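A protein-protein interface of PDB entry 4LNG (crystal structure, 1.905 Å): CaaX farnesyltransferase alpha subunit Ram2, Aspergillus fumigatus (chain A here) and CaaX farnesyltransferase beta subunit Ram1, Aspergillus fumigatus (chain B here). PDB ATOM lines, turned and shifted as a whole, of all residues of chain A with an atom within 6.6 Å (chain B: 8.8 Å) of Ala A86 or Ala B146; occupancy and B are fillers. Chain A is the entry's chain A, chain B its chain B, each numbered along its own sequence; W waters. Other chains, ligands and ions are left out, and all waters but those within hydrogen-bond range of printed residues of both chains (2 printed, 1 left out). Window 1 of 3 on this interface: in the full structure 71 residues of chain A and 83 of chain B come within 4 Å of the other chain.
The backbone NH of Gly B192 lies within hydrogen-bond range of the side-chain hydroxyl of Tyr A88 (3.0 Å).
The backbone carbonyl oxygen (O) of Val B145 lies within hydrogen-bond range of the side-chain amide nitrogen (ND2) of Asn A84.
O of Asp B148 is in hydrogen-bond range of NE2 of Gln B196, 3.2 Å away.
The backbone NH (N) of Ala A86 lies close to the side-chain amide oxygen (OD1) of Asn A84 (3.2 Å).
CD1 of Ile A47 touches O of Phe B144, 3.4 Å away.
Leu B147 touches Ile A47 (C to CD1, 3.98 Å).
Ile A47 touches Asp B148 (CD1 to N, 3.8 Å).
Val B145 touches Met A83.
Ala A86 touches Ala B146.
Ala A86 touches Ala B149 (O to CB, 3.6 Å).
CD2 of Tyr A88 touches CB of Ala B149 (3.6 Å).
Tyr A88 touches Gln B196.
Tyr A88 touches His B199 (OH to CB, 3.5 Å).
Gln B196 touches Thr A89 (CA to OG1, 3.5 Å).
No residue of chain B comes within 4 Å of Pro A85.
Of the printed residues of chain B, Ala A86 touches Ala B146 (3.9 Å) and Ala B149 (3.6 Å).
Val A90 touches none of the printed residues of chain B.
Printed residues of chain A within 4 Å of Ala B146: Asn A84 and Ala A86.
Of the printed residues of chain A, Leu B147 touches Ile A47.
Of the printed residues of chain A, Asp B148 touches Ile A47 (3.8 Å).
Met B154 touches none of the printed residues of chain A.
The nearest printed residue of chain B that does not touch Ala A86 is Ser B150 (6.0 Å).
The nearest residue of chain A that does not touch Ala B146 is Ile A47 (5.8 Å).
Of the 15 printed residues of chain B, 10 touch a printed residue of chain A.
Printed residues of chain B that touch a printed residue of chain A: Pro B141, Phe B144, Val B145, Ala B146, Leu B147, Asp B148, Ala B149, Gly B192, Gln B196 and His B199.
Of the 13 printed residues of chain A, 6 touch a printed residue of chain B.
Among the printed residues, 14 pairs touch across the chains.
Among the printed residues, no Asp or Glu carboxylate lies within 4 Å of a Lys or Arg side-chain nitrogen of the other chain.
Water W2 lies within hydrogen-bond range of OE1 of Gln B196, OG1 of Thr A89 and ND1 of His A87.
Water W1 bridges the backbone NH (N) of Ile A47 (3.0 Å) and the guanidinium group (NE) of Arg B151 (3.4 Å).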
ATOM      1  N   ILE A  47       8.101  31.542  23.649  1.00  0.00           N
ATOM      2  CA  ILE A  47       9.029  32.541  23.135  1.00  0.00           C
ATOM      3  C   ILE A  47       8.243  33.743  22.633  1.00  0.00           C
ATOM      4  O   ILE A  47       7.322  33.598  21.829  1.00  0.00           O
ATOM      5  CB  ILE A  47       9.879  31.972  21.982  1.00  0.00           C
ATOM      6  CG1 ILE A  47      10.647  30.731  22.443  1.00  0.00           C
ATOM      7  CG2 ILE A  47      10.832  33.033  21.443  1.00  0.00           C
ATOM      8  CD1 ILE A  47      11.249  29.923  21.304  1.00  0.00           C
ATOM      9  N   ILE A  81      14.002  31.786   6.797  1.00  0.00           N
ATOM     10  CA  ILE A  81      15.346  31.246   6.980  1.00  0.00           C
ATOM     11  C   ILE A  81      16.323  32.327   7.448  1.00  0.00           C
ATOM     12  O   ILE A  81      17.217  32.058   8.255  1.00  0.00           O
ATOM     13  CB  ILE A  81      15.858  30.548   5.693  1.00  0.00           C
ATOM     14  CG1 ILE A  81      15.157  29.197   5.518  1.00  0.00           C
ATOM     15  CG2 ILE A  81      17.370  30.338   5.738  1.00  0.00           C
ATOM     16  CD1 ILE A  81      15.382  28.550   4.164  1.00  0.00           C
ATOM     17  N   MET A  83      15.599  34.743   9.356  1.00  0.00           N
ATOM     18  CA  MET A  83      15.292  35.001  10.761  1.00  0.00           C
ATOM     19  C   MET A  83      15.608  33.802  11.650  1.00  0.00           C
ATOM     20  O   MET A  83      16.024  33.961  12.797  1.00  0.00           O
ATOM     21  CB  MET A  83      13.824  35.395  10.930  1.00  0.00           C
ATOM     22  CG  MET A  83      13.494  36.795  10.441  1.00  0.00           C
ATOM     23  SD  MET A  83      11.762  37.226  10.698  1.00  0.00           S
ATOM     24  CE  MET A  83      10.973  36.258   9.420  1.00  0.00           C
ATOM     25  N   ASN A  84      15.402  32.600  11.122  1.00  0.00           N
ATOM     26  CA  ASN A  84      15.592  31.381  11.899  1.00  0.00           C
ATOM     27  C   ASN A  84      15.973  30.193  11.023  1.00  0.00           C
ATOM     28  O   ASN A  84      15.106  29.440  10.578  1.00  0.00           O
ATOM     29  CB  ASN A  84      14.327  31.057  12.694  1.00  0.00           C
ATOM     30  CG  ASN A  84      14.450  29.769  13.487  1.00  0.00           C
ATOM     31  OD1 ASN A  84      15.554  29.304  13.775  1.00  0.00           O
ATOM     32  ND2 ASN A  84      13.310  29.183  13.841  1.00  0.00           N
ATOM     33  N   PRO A  85      17.278  30.016  10.781  1.00  0.00           N
ATOM     34  CA  PRO A  85      17.772  28.928   9.925  1.00  0.00           C
ATOM     35  C   PRO A  85      17.615  27.542  10.550  1.00  0.00           C
ATOM     36  O   PRO A  85      17.821  26.544   9.863  1.00  0.00           O
ATOM     37  CB  PRO A  85      19.254  29.274   9.733  1.00  0.00           C
ATOM     38  CG  PRO A  85      19.602  30.143  10.894  1.00  0.00           C
ATOM     39  CD  PRO A  85      18.359  30.918  11.220  1.00  0.00           C
ATOM     40  N   ALA A  86      17.243  27.477  11.825  1.00  0.00           N
ATOM     41  CA  ALA A  86      17.019  26.190  12.481  1.00  0.00           C
ATOM     42  C   ALA A  86      15.555  25.748  12.408  1.00  0.00           C
ATOM     43  O   ALA A  86      15.129  24.858  13.144  1.00  0.00           O
ATOM     44  CB  ALA A  86      17.492  26.242  13.928  1.00  0.00           C
ATOM     45  N   HIS A  87      14.788  26.377  11.522  1.00  0.00           N
ATOM     46  CA  HIS A  87      13.391  26.015  11.303  1.00  0.00           C
ATOM     47  C   HIS A  87      13.338  24.859  10.304  1.00  0.00           C
ATOM     48  O   HIS A  87      13.327  25.086   9.095  1.00  0.00           O
ATOM     49  CB  HIS A  87      12.643  27.234  10.751  1.00  0.00           C
ATOM     50  CG  HIS A  87      11.149  27.117  10.787  1.00  0.00           C
ATOM     51  ND1 HIS A  87      10.456  26.159  10.079  1.00  0.00           N
ATOM     52  CD2 HIS A  87      10.214  27.868  11.416  1.00  0.00           C
ATOM     53  CE1 HIS A  87       9.160  26.310  10.288  1.00  0.00           C
ATOM     54  NE2 HIS A  87       8.985  27.339  11.096  1.00  0.00           N
ATOM     55  N   TYR A  88      13.312  23.622  10.799  1.00  0.00           N
ATOM     56  CA  TYR A  88      13.428  22.451   9.923  1.00  0.00           C
ATOM     57  C   TYR A  88      12.311  22.352   8.883  1.00  0.00           C
ATOM     58  O   TYR A  88      12.548  21.941   7.745  1.00  0.00           O
ATOM     59  CB  TYR A  88      13.546  21.141  10.729  1.00  0.00           C
ATOM     60  CG  TYR A  88      12.342  20.804  11.586  1.00  0.00           C
ATOM     61  CD1 TYR A  88      11.272  20.081  11.068  1.00  0.00           C
ATOM     62  CD2 TYR A  88      12.281  21.201  12.916  1.00  0.00           C
ATOM     63  CE1 TYR A  88      10.167  19.775  11.849  1.00  0.00           C
ATOM     64  CE2 TYR A  88      11.180  20.897  13.705  1.00  0.00           C
ATOM     65  CZ  TYR A  88      10.128  20.184  13.163  1.00  0.00           C
ATOM     66  OH  TYR A  88       9.033  19.882  13.941  1.00  0.00           O
ATOM     67  N   THR A  89      11.100  22.730   9.275  1.00  0.00           N
ATOM     68  CA  THR A  89       9.946  22.644   8.388  1.00  0.00           C
ATOM     69  C   THR A  89      10.107  23.506   7.132  1.00  0.00           C
ATOM     70  O   THR A  89       9.781  23.076   6.026  1.00  0.00           O
ATOM     71  CB  THR A  89       8.654  23.051   9.119  1.00  0.00           C
ATOM     72  OG1 THR A  89       8.451  22.182  10.241  1.00  0.00           O
ATOM     73  CG2 THR A  89       7.451  22.969   8.188  1.00  0.00           C
ATOM     74  N   VAL A  90      10.625  24.717   7.306  1.00  0.00           N
ATOM     75  CA  VAL A  90      10.699  25.659   6.198  1.00  0.00           C
ATOM     76  C   VAL A  90      11.690  25.214   5.116  1.00  0.00           C
ATOM     77  O   VAL A  90      11.458  25.445   3.927  1.00  0.00           O
ATOM     78  CB  VAL A  90      10.983  27.106   6.687  1.00  0.00           C
ATOM     79  CG1 VAL A  90      12.440  27.284   7.063  1.00  0.00           C
ATOM     80  CG2 VAL A  90      10.586  28.111   5.620  1.00  0.00           C
ATOM     81  N   TRP A  91      12.774  24.556   5.526  1.00  0.00           N
ATOM     82  CA  TRP A  91      13.769  24.032   4.589  1.00  0.00           C
ATOM     83  C   TRP A  91      13.184  22.949   3.692  1.00  0.00           C
ATOM     84  O   TRP A  91      13.434  22.911   2.485  1.00  0.00           O
ATOM     85  CB  TRP A  91      14.969  23.455   5.343  1.00  0.00           C
ATOM     86  CG  TRP A  91      15.920  24.488   5.851  1.00  0.00           C
ATOM     87  CD1 TRP A  91      16.064  24.906   7.142  1.00  0.00           C
ATOM     88  CD2 TRP A  91      16.864  25.233   5.077  1.00  0.00           C
ATOM     89  NE1 TRP A  91      17.045  25.866   7.221  1.00  0.00           N
ATOM     90  CE2 TRP A  91      17.550  26.087   5.964  1.00  0.00           C
ATOM     91  CE3 TRP A  91      17.199  25.261   3.719  1.00  0.00           C
ATOM     92  CZ2 TRP A  91      18.549  26.960   5.538  1.00  0.00           C
ATOM     93  CZ3 TRP A  91      18.191  26.128   3.297  1.00  0.00           C
ATOM     94  CH2 TRP A  91      18.855  26.967   4.203  1.00  0.00           C
ATOM     95  N   ASN A 122      25.155  25.374  11.717  1.00  0.00           N
ATOM     96  CA  ASN A 122      23.820  24.917  11.325  1.00  0.00           C
ATOM     97  C   ASN A 122      23.885  23.676  10.442  1.00  0.00           C
ATOM     98  O   ASN A 122      24.547  23.689   9.408  1.00  0.00           O
ATOM     99  CB  ASN A 122      23.074  26.032  10.593  1.00  0.00           C
ATOM    100  CG  ASN A 122      21.660  25.634  10.207  1.00  0.00           C
ATOM    101  OD1 ASN A 122      21.450  24.869   9.265  1.00  0.00           O
ATOM    102  ND2 ASN A 122      20.683  26.159  10.930  1.00  0.00           N
ATOM    103  N   GLN A 124      20.992  21.903   9.276  1.00  0.00           N
ATOM    104  CA  GLN A 124      19.855  21.842   8.355  1.00  0.00           C
ATOM    105  C   GLN A 124      20.253  22.260   6.937  1.00  0.00           C
ATOM    106  O   GLN A 124      19.776  21.694   5.947  1.00  0.00           O
ATOM    107  CB  GLN A 124      18.706  22.730   8.844  1.00  0.00           C
ATOM    108  CG  GLN A 124      17.935  22.183  10.039  1.00  0.00           C
ATOM    109  CD  GLN A 124      18.569  22.542  11.369  1.00  0.00           C
ATOM    110  OE1 GLN A 124      19.578  23.244  11.423  1.00  0.00           O
ATOM    111  NE2 GLN A 124      17.974  22.060  12.455  1.00  0.00           N
ATOM    112  N   PRO B 141      12.658  35.772  25.704  1.00  0.00           N
ATOM    113  CA  PRO B 141      12.605  36.932  24.806  1.00  0.00           C
ATOM    114  C   PRO B 141      12.788  36.538  23.340  1.00  0.00           C
ATOM    115  O   PRO B 141      13.128  35.391  23.046  1.00  0.00           O
ATOM    116  CB  PRO B 141      13.779  37.797  25.281  1.00  0.00           C
ATOM    117  CG  PRO B 141      14.711  36.842  25.938  1.00  0.00           C
ATOM    118  CD  PRO B 141      13.838  35.808  26.584  1.00  0.00           C
ATOM    119  N   ALA B 142      12.567  37.494  22.441  1.00  0.00           N
ATOM    120  CA  ALA B 142      12.580  37.239  21.000  1.00  0.00           C
ATOM    121  C   ALA B 142      13.902  36.675  20.490  1.00  0.00           C
ATOM    122  O   ALA B 142      13.938  35.981  19.473  1.00  0.00           O
ATOM    123  CB  ALA B 142      12.217  38.505  20.236  1.00  0.00           C
ATOM    124  N   SER B 143      14.985  36.968  21.202  1.00  0.00           N
ATOM    125  CA  SER B 143      16.313  36.511  20.805  1.00  0.00           C
ATOM    126  C   SER B 143      16.452  34.990  20.827  1.00  0.00           C
ATOM    127  O   SER B 143      17.394  34.441  20.258  1.00  0.00           O
ATOM    128  CB  SER B 143      17.383  37.148  21.696  1.00  0.00           C
ATOM    129  OG  SER B 143      17.179  36.809  23.058  1.00  0.00           O
ATOM    130  N   PHE B 144      15.516  34.310  21.481  1.00  0.00           N
ATOM    131  CA  PHE B 144      15.558  32.852  21.569  1.00  0.00           C
ATOM    132  C   PHE B 144      14.783  32.166  20.443  1.00  0.00           C
ATOM    133  O   PHE B 144      14.439  30.985  20.551  1.00  0.00           O
ATOM    134  CB  PHE B 144      15.050  32.378  22.935  1.00  0.00           C
ATOM    135  CG  PHE B 144      16.072  32.494  24.032  1.00  0.00           C
ATOM    136  CD1 PHE B 144      16.315  33.711  24.645  1.00  0.00           C
ATOM    137  CD2 PHE B 144      16.791  31.386  24.447  1.00  0.00           C
ATOM    138  CE1 PHE B 144      17.257  33.819  25.650  1.00  0.00           C
ATOM    139  CE2 PHE B 144      17.732  31.489  25.452  1.00  0.00           C
ATOM    140  CZ  PHE B 144      17.965  32.706  26.053  1.00  0.00           C
ATOM    141  N   VAL B 145      14.531  32.902  19.363  1.00  0.00           N
ATOM    142  CA  VAL B 145      13.766  32.388  18.229  1.00  0.00           C
ATOM    143  C   VAL B 145      14.384  31.116  17.637  1.00  0.00           C
ATOM    144  O   VAL B 145      13.682  30.278  17.071  1.00  0.00           O
ATOM    145  CB  VAL B 145      13.591  33.471  17.127  1.00  0.00           C
ATOM    146  CG1 VAL B 145      14.930  33.810  16.482  1.00  0.00           C
ATOM    147  CG2 VAL B 145      12.583  33.025  16.078  1.00  0.00           C
ATOM    148  N   ALA B 146      15.696  30.960  17.792  1.00  0.00           N
ATOM    149  CA  ALA B 146      16.394  29.783  17.274  1.00  0.00           C
ATOM    150  C   ALA B 146      15.911  28.481  17.909  1.00  0.00           C
ATOM    151  O   ALA B 146      16.109  27.403  17.352  1.00  0.00           O
ATOM    152  CB  ALA B 146      17.901  29.934  17.455  1.00  0.00           C
ATOM    153  N   LEU B 147      15.280  28.582  19.076  1.00  0.00           N
ATOM    154  CA  LEU B 147      14.775  27.406  19.775  1.00  0.00           C
ATOM    155  C   LEU B 147      13.319  27.086  19.430  1.00  0.00           C
ATOM    156  O   LEU B 147      12.745  26.145  19.978  1.00  0.00           O
ATOM    157  CB  LEU B 147      14.920  27.584  21.290  1.00  0.00           C
ATOM    158  CG  LEU B 147      16.353  27.616  21.826  1.00  0.00           C
ATOM    159  CD1 LEU B 147      16.365  27.871  23.330  1.00  0.00           C
ATOM    160  CD2 LEU B 147      17.068  26.317  21.495  1.00  0.00           C
ATOM    161  N   ASP B 148      12.735  27.860  18.520  1.00  0.00           N
ATOM    162  CA  ASP B 148      11.319  27.719  18.165  1.00  0.00           C
ATOM    163  C   ASP B 148      10.949  26.299  17.740  1.00  0.00           C
ATOM    164  O   ASP B 148       9.885  25.795  18.097  1.00  0.00           O
ATOM    165  CB  ASP B 148      10.943  28.706  17.055  1.00  0.00           C
ATOM    166  CG  ASP B 148       9.458  28.682  16.723  1.00  0.00           C
ATOM    167  OD1 ASP B 148       8.639  28.452  17.637  1.00  0.00           O
ATOM    168  OD2 ASP B 148       9.109  28.906  15.544  1.00  0.00           O
ATOM    169  N   ALA B 149      11.827  25.653  16.980  1.00  0.00           N
ATOM    170  CA  ALA B 149      11.547  24.302  16.498  1.00  0.00           C
ATOM    171  C   ALA B 149      11.895  23.233  17.530  1.00  0.00           C
ATOM    172  O   ALA B 149      11.672  22.043  17.298  1.00  0.00           O
ATOM    173  CB  ALA B 149      12.286  24.039  15.194  1.00  0.00           C
ATOM    174  N   SER B 150      12.427  23.655  18.674  1.00  0.00           N
ATOM    175  CA  SER B 150      12.871  22.724  19.706  1.00  0.00           C
ATOM    176  C   SER B 150      12.177  22.944  21.051  1.00  0.00           C
ATOM    177  O   SER B 150      12.677  22.516  22.089  1.00  0.00           O
ATOM    178  CB  SER B 150      14.389  22.824  19.887  1.00  0.00           C
ATOM    179  OG  SER B 150      15.065  22.538  18.676  1.00  0.00           O
ATOM    180  N   ARG B 151      11.033  23.615  21.035  1.00  0.00           N
ATOM    181  CA  ARG B 151      10.296  23.863  22.275  1.00  0.00           C
ATOM    182  C   ARG B 151       9.895  22.600  23.060  1.00  0.00           C
ATOM    183  O   ARG B 151       9.949  22.608  24.288  1.00  0.00           O
ATOM    184  CB  ARG B 151       9.099  24.791  22.042  1.00  0.00           C
ATOM    185  CG  ARG B 151       9.491  26.266  21.967  1.00  0.00           C
ATOM    186  CD  ARG B 151       8.282  27.186  21.811  1.00  0.00           C
ATOM    187  NE  ARG B 151       7.324  27.018  22.900  1.00  0.00           N
ATOM    188  CZ  ARG B 151       6.069  26.619  22.735  1.00  0.00           C
ATOM    189  NH1 ARG B 151       5.608  26.358  21.517  1.00  0.00           N
ATOM    190  NH2 ARG B 151       5.271  26.489  23.785  1.00  0.00           N
ATOM    191  N   MET B 154      12.774  21.655  25.209  1.00  0.00           N
ATOM    192  CA  MET B 154      12.954  22.534  26.360  1.00  0.00           C
ATOM    193  C   MET B 154      12.069  22.121  27.531  1.00  0.00           C
ATOM    194  O   MET B 154      12.471  22.229  28.691  1.00  0.00           O
ATOM    195  CB  MET B 154      12.691  23.988  25.972  1.00  0.00           C
ATOM    196  CG  MET B 154      13.539  24.457  24.802  1.00  0.00           C
ATOM    197  SD  MET B 154      13.096  26.111  24.246  1.00  0.00           S
ATOM    198  CE  MET B 154      13.542  27.064  25.686  1.00  0.00           C
ATOM    199  N   GLY B 192       7.652  20.813  16.394  1.00  0.00           N
ATOM    200  CA  GLY B 192       8.219  21.801  17.297  1.00  0.00           C
ATOM    201  C   GLY B 192       7.208  22.807  17.821  1.00  0.00           C
ATOM    202  O   GLY B 192       7.464  23.498  18.808  1.00  0.00           O
ATOM    203  N   GLN B 196       4.329  23.366  12.505  1.00  0.00           N
ATOM    204  CA  GLN B 196       5.568  22.677  12.163  1.00  0.00           C
ATOM    205  C   GLN B 196       5.281  21.200  11.929  1.00  0.00           C
ATOM    206  O   GLN B 196       4.480  20.601  12.641  1.00  0.00           O
ATOM    207  CB  GLN B 196       6.620  22.846  13.263  1.00  0.00           C
ATOM    208  CG  GLN B 196       6.785  24.277  13.749  1.00  0.00           C
ATOM    209  CD  GLN B 196       7.998  24.450  14.642  1.00  0.00           C
ATOM    210  OE1 GLN B 196       9.053  23.868  14.391  1.00  0.00           O
ATOM    211  NE2 GLN B 196       7.853  25.250  15.691  1.00  0.00           N
ATOM    212  N   HIS B 199       8.155  15.593  13.886  1.00  0.00           N
ATOM    213  CA  HIS B 199       9.578  15.300  13.927  1.00  0.00           C
ATOM    214  C   HIS B 199       9.771  14.297  15.059  1.00  0.00           C
ATOM    215  O   HIS B 199       9.149  14.436  16.116  1.00  0.00           O
ATOM    216  CB  HIS B 199      10.345  16.601  14.195  1.00  0.00           C
ATOM    217  CG  HIS B 199      11.831  16.490  14.042  1.00  0.00           C
ATOM    218  ND1 HIS B 199      12.626  15.821  14.948  1.00  0.00           N
ATOM    219  CD2 HIS B 199      12.670  16.991  13.105  1.00  0.00           C
ATOM    220  CE1 HIS B 199      13.889  15.903  14.567  1.00  0.00           C
ATOM    221  NE2 HIS B 199      13.943  16.608  13.452  1.00  0.00           N
HETATM  222  O   HOH W   1       6.253  30.057  21.848  1.00  0.00           O
HETATM  223  O   HOH W   2      10.001  23.451  12.040  1.00  0.00           O
